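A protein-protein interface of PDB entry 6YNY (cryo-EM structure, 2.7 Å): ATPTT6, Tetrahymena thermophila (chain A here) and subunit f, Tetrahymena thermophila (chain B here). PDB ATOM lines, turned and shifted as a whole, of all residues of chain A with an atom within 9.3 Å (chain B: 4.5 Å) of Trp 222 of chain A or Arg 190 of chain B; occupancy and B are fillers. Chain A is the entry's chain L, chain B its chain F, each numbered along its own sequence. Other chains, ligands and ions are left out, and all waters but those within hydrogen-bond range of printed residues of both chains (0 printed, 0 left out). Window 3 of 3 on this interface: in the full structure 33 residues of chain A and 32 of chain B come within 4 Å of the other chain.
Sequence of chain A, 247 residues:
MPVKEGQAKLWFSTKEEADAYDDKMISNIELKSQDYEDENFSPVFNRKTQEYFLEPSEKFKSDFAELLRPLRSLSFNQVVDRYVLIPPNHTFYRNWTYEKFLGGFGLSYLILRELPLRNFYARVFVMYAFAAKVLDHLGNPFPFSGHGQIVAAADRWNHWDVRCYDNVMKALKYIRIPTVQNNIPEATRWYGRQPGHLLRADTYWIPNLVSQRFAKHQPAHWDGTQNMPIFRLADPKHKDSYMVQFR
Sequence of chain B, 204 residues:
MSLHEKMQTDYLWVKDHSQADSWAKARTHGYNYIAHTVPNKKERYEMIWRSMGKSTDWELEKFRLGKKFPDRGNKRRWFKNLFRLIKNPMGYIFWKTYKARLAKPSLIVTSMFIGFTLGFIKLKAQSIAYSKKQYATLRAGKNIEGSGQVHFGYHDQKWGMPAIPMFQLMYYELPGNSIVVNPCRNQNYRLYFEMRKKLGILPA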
ATOM      1  N   PRO A 219       4.992  17.916   3.381  1.00  0.00           N
ATOM      2  CA  PRO A 219       4.956  16.458   3.233  1.00  0.00           C
ATOM      3  C   PRO A 219       5.167  15.759   4.568  1.00  0.00           C
ATOM      4  O   PRO A 219       6.065  16.110   5.335  1.00  0.00           O
ATOM      5  CB  PRO A 219       6.102  16.174   2.258  1.00  0.00           C
ATOM      6  CG  PRO A 219       7.007  17.330   2.393  1.00  0.00           C
ATOM      7  CD  PRO A 219       6.143  18.508   2.684  1.00  0.00           C
ATOM      8  N   ALA A 220       4.324  14.769   4.838  1.00  0.00           N
ATOM      9  CA  ALA A 220       4.431  13.939   6.034  1.00  0.00           C
ATOM     10  C   ALA A 220       5.163  12.665   5.638  1.00  0.00           C
ATOM     11  O   ALA A 220       4.570  11.744   5.072  1.00  0.00           O
ATOM     12  CB  ALA A 220       3.056  13.640   6.617  1.00  0.00           C
ATOM     13  N   HIS A 221       6.457  12.617   5.932  1.00  0.00           N
ATOM     14  CA  HIS A 221       7.276  11.487   5.523  1.00  0.00           C
ATOM     15  C   HIS A 221       6.962  10.265   6.373  1.00  0.00           C
ATOM     16  O   HIS A 221       7.018  10.315   7.605  1.00  0.00           O
ATOM     17  CB  HIS A 221       8.750  11.848   5.619  1.00  0.00           C
ATOM     18  CG  HIS A 221       9.155  12.950   4.694  1.00  0.00           C
ATOM     19  ND1 HIS A 221       9.528  12.723   3.387  1.00  0.00           N
ATOM     20  CD2 HIS A 221       9.240  14.287   4.883  1.00  0.00           C
ATOM     21  CE1 HIS A 221       9.829  13.873   2.812  1.00  0.00           C
ATOM     22  NE2 HIS A 221       9.663  14.837   3.698  1.00  0.00           N
ATOM     23  N   TRP A 222       6.647   9.163   5.703  1.00  0.00           N
ATOM     24  CA  TRP A 222       6.238   7.944   6.382  1.00  0.00           C
ATOM     25  C   TRP A 222       7.357   7.413   7.266  1.00  0.00           C
ATOM     26  O   TRP A 222       8.492   7.235   6.814  1.00  0.00           O
ATOM     27  CB  TRP A 222       5.829   6.904   5.345  1.00  0.00           C
ATOM     28  CG  TRP A 222       5.276   5.649   5.903  1.00  0.00           C
ATOM     29  CD1 TRP A 222       4.309   5.528   6.849  1.00  0.00           C
ATOM     30  CD2 TRP A 222       5.640   4.320   5.531  1.00  0.00           C
ATOM     31  NE1 TRP A 222       4.051   4.206   7.098  1.00  0.00           N
ATOM     32  CE2 TRP A 222       4.858   3.442   6.300  1.00  0.00           C
ATOM     33  CE3 TRP A 222       6.556   3.786   4.626  1.00  0.00           C
ATOM     34  CZ2 TRP A 222       4.964   2.064   6.192  1.00  0.00           C
ATOM     35  CZ3 TRP A 222       6.660   2.419   4.521  1.00  0.00           C
ATOM     36  CH2 TRP A 222       5.870   1.573   5.299  1.00  0.00           C
ATOM     37  N   ASP A 223       7.032   7.164   8.533  1.00  0.00           N
ATOM     38  CA  ASP A 223       7.989   6.669   9.510  1.00  0.00           C
ATOM     39  C   ASP A 223       7.914   5.161   9.702  1.00  0.00           C
ATOM     40  O   ASP A 223       8.597   4.627  10.580  1.00  0.00           O
ATOM     41  CB  ASP A 223       7.781   7.371  10.850  1.00  0.00           C
ATOM     42  CG  ASP A 223       6.423   7.087  11.456  1.00  0.00           C
ATOM     43  OD1 ASP A 223       5.571   6.494  10.764  1.00  0.00           O
ATOM     44  OD2 ASP A 223       6.209   7.454  12.629  1.00  0.00           O
ATOM     45  N   GLY A 224       7.104   4.466   8.914  1.00  0.00           N
ATOM     46  CA  GLY A 224       6.994   3.028   9.008  1.00  0.00           C
ATOM     47  C   GLY A 224       5.840   2.523   9.837  1.00  0.00           C
ATOM     48  O   GLY A 224       5.797   1.325  10.135  1.00  0.00           O
ATOM     49  N   THR A 225       4.905   3.387  10.212  1.00  0.00           N
ATOM     50  CA  THR A 225       3.781   3.027  11.058  1.00  0.00           C
ATOM     51  C   THR A 225       2.475   3.217  10.301  1.00  0.00           C
ATOM     52  O   THR A 225       2.440   3.744   9.188  1.00  0.00           O
ATOM     53  CB  THR A 225       3.765   3.864  12.342  1.00  0.00           C
ATOM     54  OG1 THR A 225       3.618   5.250  12.015  1.00  0.00           O
ATOM     55  CG2 THR A 225       5.042   3.671  13.105  1.00  0.00           C
ATOM     56  N   GLN A 226       1.394   2.770  10.932  1.00  0.00           N
ATOM     57  CA  GLN A 226       0.049   2.902  10.394  1.00  0.00           C
ATOM     58  C   GLN A 226      -0.824   3.819  11.237  1.00  0.00           C
ATOM     59  O   GLN A 226      -2.039   3.867  11.029  1.00  0.00           O
ATOM     60  CB  GLN A 226      -0.602   1.525  10.277  1.00  0.00           C
ATOM     61  CG  GLN A 226       0.038   0.636   9.243  1.00  0.00           C
ATOM     62  CD  GLN A 226      -0.158   1.152   7.839  1.00  0.00           C
ATOM     63  OE1 GLN A 226      -1.170   1.779   7.532  1.00  0.00           O
ATOM     64  NE2 GLN A 226       0.814   0.903   6.981  1.00  0.00           N
ATOM     65  N   ASN A 227      -0.230   4.553  12.178  1.00  0.00           N
ATOM     66  CA  ASN A 227      -0.983   5.373  13.116  1.00  0.00           C
ATOM     67  C   ASN A 227      -0.444   6.797  13.189  1.00  0.00           C
ATOM     68  O   ASN A 227      -0.682   7.490  14.181  1.00  0.00           O
ATOM     69  CB  ASN A 227      -0.960   4.737  14.503  1.00  0.00           C
ATOM     70  CG  ASN A 227       0.441   4.477  14.996  1.00  0.00           C
ATOM     71  OD1 ASN A 227       1.415   4.944  14.411  1.00  0.00           O
ATOM     72  ND2 ASN A 227       0.552   3.733  16.080  1.00  0.00           N
ATOM     73  N   MET A 228       0.266   7.246  12.165  1.00  0.00           N
ATOM     74  CA  MET A 228       0.859   8.575  12.168  1.00  0.00           C
ATOM     75  C   MET A 228      -0.225   9.632  12.333  1.00  0.00           C
ATOM     76  O   MET A 228      -1.061   9.804  11.439  1.00  0.00           O
ATOM     77  CB  MET A 228       1.637   8.815  10.878  1.00  0.00           C
ATOM     78  CG  MET A 228       2.786   7.865  10.668  1.00  0.00           C
ATOM     79  SD  MET A 228       3.650   8.165   9.123  1.00  0.00           S
ATOM     80  CE  MET A 228       4.263   9.813   9.419  1.00  0.00           C
ATOM     81  N   ILE A 230      -1.056  12.579  11.551  1.00  0.00           N
ATOM     82  CA  ILE A 230      -0.835  13.742  10.698  1.00  0.00           C
ATOM     83  C   ILE A 230      -2.042  14.659  10.650  1.00  0.00           C
ATOM     84  O   ILE A 230      -1.954  15.761  10.095  1.00  0.00           O
ATOM     85  CB  ILE A 230      -0.449  13.299   9.275  1.00  0.00           C
ATOM     86  CG1 ILE A 230      -1.598  12.544   8.613  1.00  0.00           C
ATOM     87  CG2 ILE A 230       0.782  12.439   9.320  1.00  0.00           C
ATOM     88  CD1 ILE A 230      -1.219  11.886   7.328  1.00  0.00           C
ATOM     89  N   CYS B 184      -1.507   6.181   5.799  1.00  0.00           N
ATOM     90  CA  CYS B 184      -0.424   5.210   5.843  1.00  0.00           C
ATOM     91  C   CYS B 184      -0.833   3.888   5.214  1.00  0.00           C
ATOM     92  O   CYS B 184       0.031   3.128   4.765  1.00  0.00           O
ATOM     93  CB  CYS B 184       0.018   4.982   7.285  1.00  0.00           C
ATOM     94  SG  CYS B 184       0.978   6.324   8.009  1.00  0.00           S
ATOM     95  N   GLN B 187       0.681   3.143   1.922  1.00  0.00           N
ATOM     96  CA  GLN B 187       2.076   2.739   1.834  1.00  0.00           C
ATOM     97  C   GLN B 187       2.246   1.234   1.707  1.00  0.00           C
ATOM     98  O   GLN B 187       3.352   0.776   1.403  1.00  0.00           O
ATOM     99  CB  GLN B 187       2.840   3.243   3.053  1.00  0.00           C
ATOM    100  CG  GLN B 187       2.682   4.723   3.295  1.00  0.00           C
ATOM    101  CD  GLN B 187       3.045   5.552   2.087  1.00  0.00           C
ATOM    102  OE1 GLN B 187       3.954   5.210   1.332  1.00  0.00           O
ATOM    103  NE2 GLN B 187       2.326   6.642   1.888  1.00  0.00           N
ATOM    104  N   ASN B 188       1.190   0.458   1.936  1.00  0.00           N
ATOM    105  CA  ASN B 188       1.251  -0.977   1.712  1.00  0.00           C
ATOM    106  C   ASN B 188       1.256  -1.329   0.234  1.00  0.00           C
ATOM    107  O   ASN B 188       1.570  -2.471  -0.113  1.00  0.00           O
ATOM    108  CB  ASN B 188       0.080  -1.661   2.407  1.00  0.00           C
ATOM    109  CG  ASN B 188       0.071  -1.421   3.893  1.00  0.00           C
ATOM    110  OD1 ASN B 188       1.113  -1.201   4.506  1.00  0.00           O
ATOM    111  ND2 ASN B 188      -1.108  -1.463   4.484  1.00  0.00           N
ATOM    112  N   TYR B 189       0.907  -0.382  -0.636  1.00  0.00           N
ATOM    113  CA  TYR B 189       0.995  -0.607  -2.069  1.00  0.00           C
ATOM    114  C   TYR B 189       2.435  -0.723  -2.539  1.00  0.00           C
ATOM    115  O   TYR B 189       2.676  -1.220  -3.643  1.00  0.00           O
ATOM    116  CB  TYR B 189       0.287   0.521  -2.813  1.00  0.00           C
ATOM    117  CG  TYR B 189      -1.214   0.418  -2.776  1.00  0.00           C
ATOM    118  CD1 TYR B 189      -1.930   0.842  -1.673  1.00  0.00           C
ATOM    119  CD2 TYR B 189      -1.914  -0.105  -3.846  1.00  0.00           C
ATOM    120  CE1 TYR B 189      -3.296   0.745  -1.635  1.00  0.00           C
ATOM    121  CE2 TYR B 189      -3.281  -0.208  -3.818  1.00  0.00           C
ATOM    122  CZ  TYR B 189      -3.971   0.219  -2.712  1.00  0.00           C
ATOM    123  OH  TYR B 189      -5.340   0.118  -2.685  1.00  0.00           O
ATOM    124  N   ARG B 190       3.391  -0.273  -1.730  1.00  0.00           N
ATOM    125  CA  ARG B 190       4.795  -0.452  -2.071  1.00  0.00           C
ATOM    126  C   ARG B 190       5.136  -1.927  -2.223  1.00  0.00           C
ATOM    127  O   ARG B 190       5.957  -2.299  -3.069  1.00  0.00           O
ATOM    128  CB  ARG B 190       5.671   0.189  -1.002  1.00  0.00           C
ATOM    129  CG  ARG B 190       5.370   1.648  -0.748  1.00  0.00           C
ATOM    130  CD  ARG B 190       6.258   2.212   0.333  1.00  0.00           C
ATOM    131  NE  ARG B 190       6.002   3.623   0.580  1.00  0.00           N
ATOM    132  CZ  ARG B 190       6.846   4.435   1.204  1.00  0.00           C
ATOM    133  NH1 ARG B 190       8.008   3.986   1.640  1.00  0.00           N
ATOM    134  NH2 ARG B 190       6.529   5.703   1.385  1.00  0.00           N
ATOM    135  N   LEU B 191       4.516  -2.782  -1.410  1.00  0.00           N
ATOM    136  CA  LEU B 191       4.713  -4.219  -1.550  1.00  0.00           C
ATOM    137  C   LEU B 191       4.318  -4.698  -2.938  1.00  0.00           C
ATOM    138  O   LEU B 191       4.978  -5.570  -3.513  1.00  0.00           O
ATOM    139  CB  LEU B 191       3.900  -4.956  -0.492  1.00  0.00           C
ATOM    140  CG  LEU B 191       4.255  -4.675   0.960  1.00  0.00           C
ATOM    141  CD1 LEU B 191       3.137  -5.124   1.867  1.00  0.00           C
ATOM    142  CD2 LEU B 191       5.533  -5.381   1.320  1.00  0.00           C
ATOM    143  N   TYR B 192       3.242  -4.143  -3.489  1.00  0.00           N
ATOM    144  CA  TYR B 192       2.776  -4.583  -4.798  1.00  0.00           C
ATOM    145  C   TYR B 192       3.755  -4.183  -5.891  1.00  0.00           C
ATOM    146  O   TYR B 192       4.042  -4.975  -6.795  1.00  0.00           O
ATOM    147  CB  TYR B 192       1.393  -4.001  -5.079  1.00  0.00           C
ATOM    148  CG  TYR B 192       0.378  -4.244  -3.989  1.00  0.00           C
ATOM    149  CD1 TYR B 192      -0.741  -3.440  -3.869  1.00  0.00           C
ATOM    150  CD2 TYR B 192       0.535  -5.275  -3.083  1.00  0.00           C
ATOM    151  CE1 TYR B 192      -1.668  -3.655  -2.880  1.00  0.00           C
ATOM    152  CE2 TYR B 192      -0.385  -5.495  -2.090  1.00  0.00           C
ATOM    153  CZ  TYR B 192      -1.485  -4.684  -1.992  1.00  0.00           C
ATOM    154  OH  TYR B 192      -2.408  -4.907  -1.002  1.00  0.00           O
ATOM    155  N   PHE B 193       4.275  -2.960  -5.827  1.00  0.00           N
ATOM    156  CA  PHE B 193       5.219  -2.501  -6.834  1.00  0.00           C
ATOM    157  C   PHE B 193       6.514  -3.295  -6.792  1.00  0.00           C
ATOM    158  O   PHE B 193       7.149  -3.499  -7.832  1.00  0.00           O
ATOM    159  CB  PHE B 193       5.498  -1.014  -6.637  1.00  0.00           C
ATOM    160  CG  PHE B 193       4.265  -0.167  -6.627  1.00  0.00           C
ATOM    161  CD1 PHE B 193       3.217  -0.438  -7.482  1.00  0.00           C
ATOM    162  CD2 PHE B 193       4.145   0.891  -5.752  1.00  0.00           C
ATOM    163  CE1 PHE B 193       2.087   0.333  -7.470  1.00  0.00           C
ATOM    164  CE2 PHE B 193       3.011   1.665  -5.738  1.00  0.00           C
ATOM    165  CZ  PHE B 193       1.982   1.385  -6.598  1.00  0.00           C
ATOM    166  N   GLU B 194       6.921  -3.750  -5.610  1.00  0.00           N
ATOM    167  CA  GLU B 194       8.146  -4.529  -5.492  1.00  0.00           C
ATOM    168  C   GLU B 194       7.946  -5.964  -5.960  1.00  0.00           C
ATOM    169  O   GLU B 194       8.857  -6.561  -6.544  1.00  0.00           O
ATOM    170  CB  GLU B 194       8.637  -4.498  -4.049  1.00  0.00           C
ATOM    171  CG  GLU B 194       8.983  -3.107  -3.555  1.00  0.00           C
ATOM    172  CD  GLU B 194       9.231  -3.059  -2.062  1.00  0.00           C
ATOM    173  OE1 GLU B 194       9.281  -4.134  -1.429  1.00  0.00           O
ATOM    174  OE2 GLU B 194       9.372  -1.945  -1.519  1.00  0.00           O
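O of Thr 225 of chain A lies within hydrogen-bond range of SG of Cys 184 of chain B, at 3.2 Å. The side-chain amide nitrogen (NE2) of Gln 226 of chain A lies within hydrogen-bond range of the backbone carbonyl oxygen (O) of Cys 184 of chain B (3.2 Å). NE2 of Gln 226 of chain A lies within hydrogen-bond range of OD1 of Asn 188 of chain B, at 3.3 Å. SG of Cys 184 of chain B sits at hydrogen-bond distance from SD of Met 228 of chain A.
The indole nitrogen (NE1) of Trp 222 of chain A is in hydrogen-bond range of the backbone carbonyl oxygen (O) of Thr 225 of chain A (2.7 Å). OD1 of Asp 223 of chain A sits at hydrogen-bond distance from OG1 of Thr 225 of chain A (2.6 Å). The backbone NH of Asp 223 of chain A is in hydrogen-bond range of the side-chain sulfur of Met 228 of chain A (3.6 Å). The side-chain hydroxyl (OG1) of Thr 225 of chain A sits at hydrogen-bond distance from the side-chain amide oxygen (OD1) of Asn 227 of chain A. NH2 of Arg 190 of chain B lies within hydrogen-bond range of OE1 of Gln 187 of chain B (2.6 Å).
Among the printed residues, merely in contact across the chains: Trp 222 of chain A with Cys 184 of chain B, Trp 222 of chain A with Gln 187 of chain B and Trp 222 of chain A with Arg 190 of chain B.
Printed residues of chain A within 4 Å of Arg 190 of chain B: Trp 222. Of the printed residues of chain B, Gln 226 of chain A touches Cys 184 (3.2 Å) and Asn 188 (3.3 Å). Of the printed residues of chain A, Cys 184 of chain B touches Trp 222 (3.6 Å), Thr 225 (3.2 Å), Gln 226 (3.2 Å) and Met 228 (3.4 Å). Gly 224 of chain A touches none of the printed residues of chain B. Asn 227 of chain A touches none of the printed residues of chain B. The nearest residue of chain A that does not touch Arg 190 of chain B is His 221 of chain A (6.8 Å). The nearest printed residue of chain A that does not touch Asn 188 of chain B is Trp 222 of chain A (5.3 Å).
Hydrophobic or aromatic side chains of chain A that line the printed part of chain B: Trp 222 and Met 228. Of the 9 printed residues of chain B, 4 touch a printed residue of chain A. Among the printed residues, no Asp or Glu carboxylate lies within 4 Å of a Lys or Arg side-chain nitrogen of the other chain.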
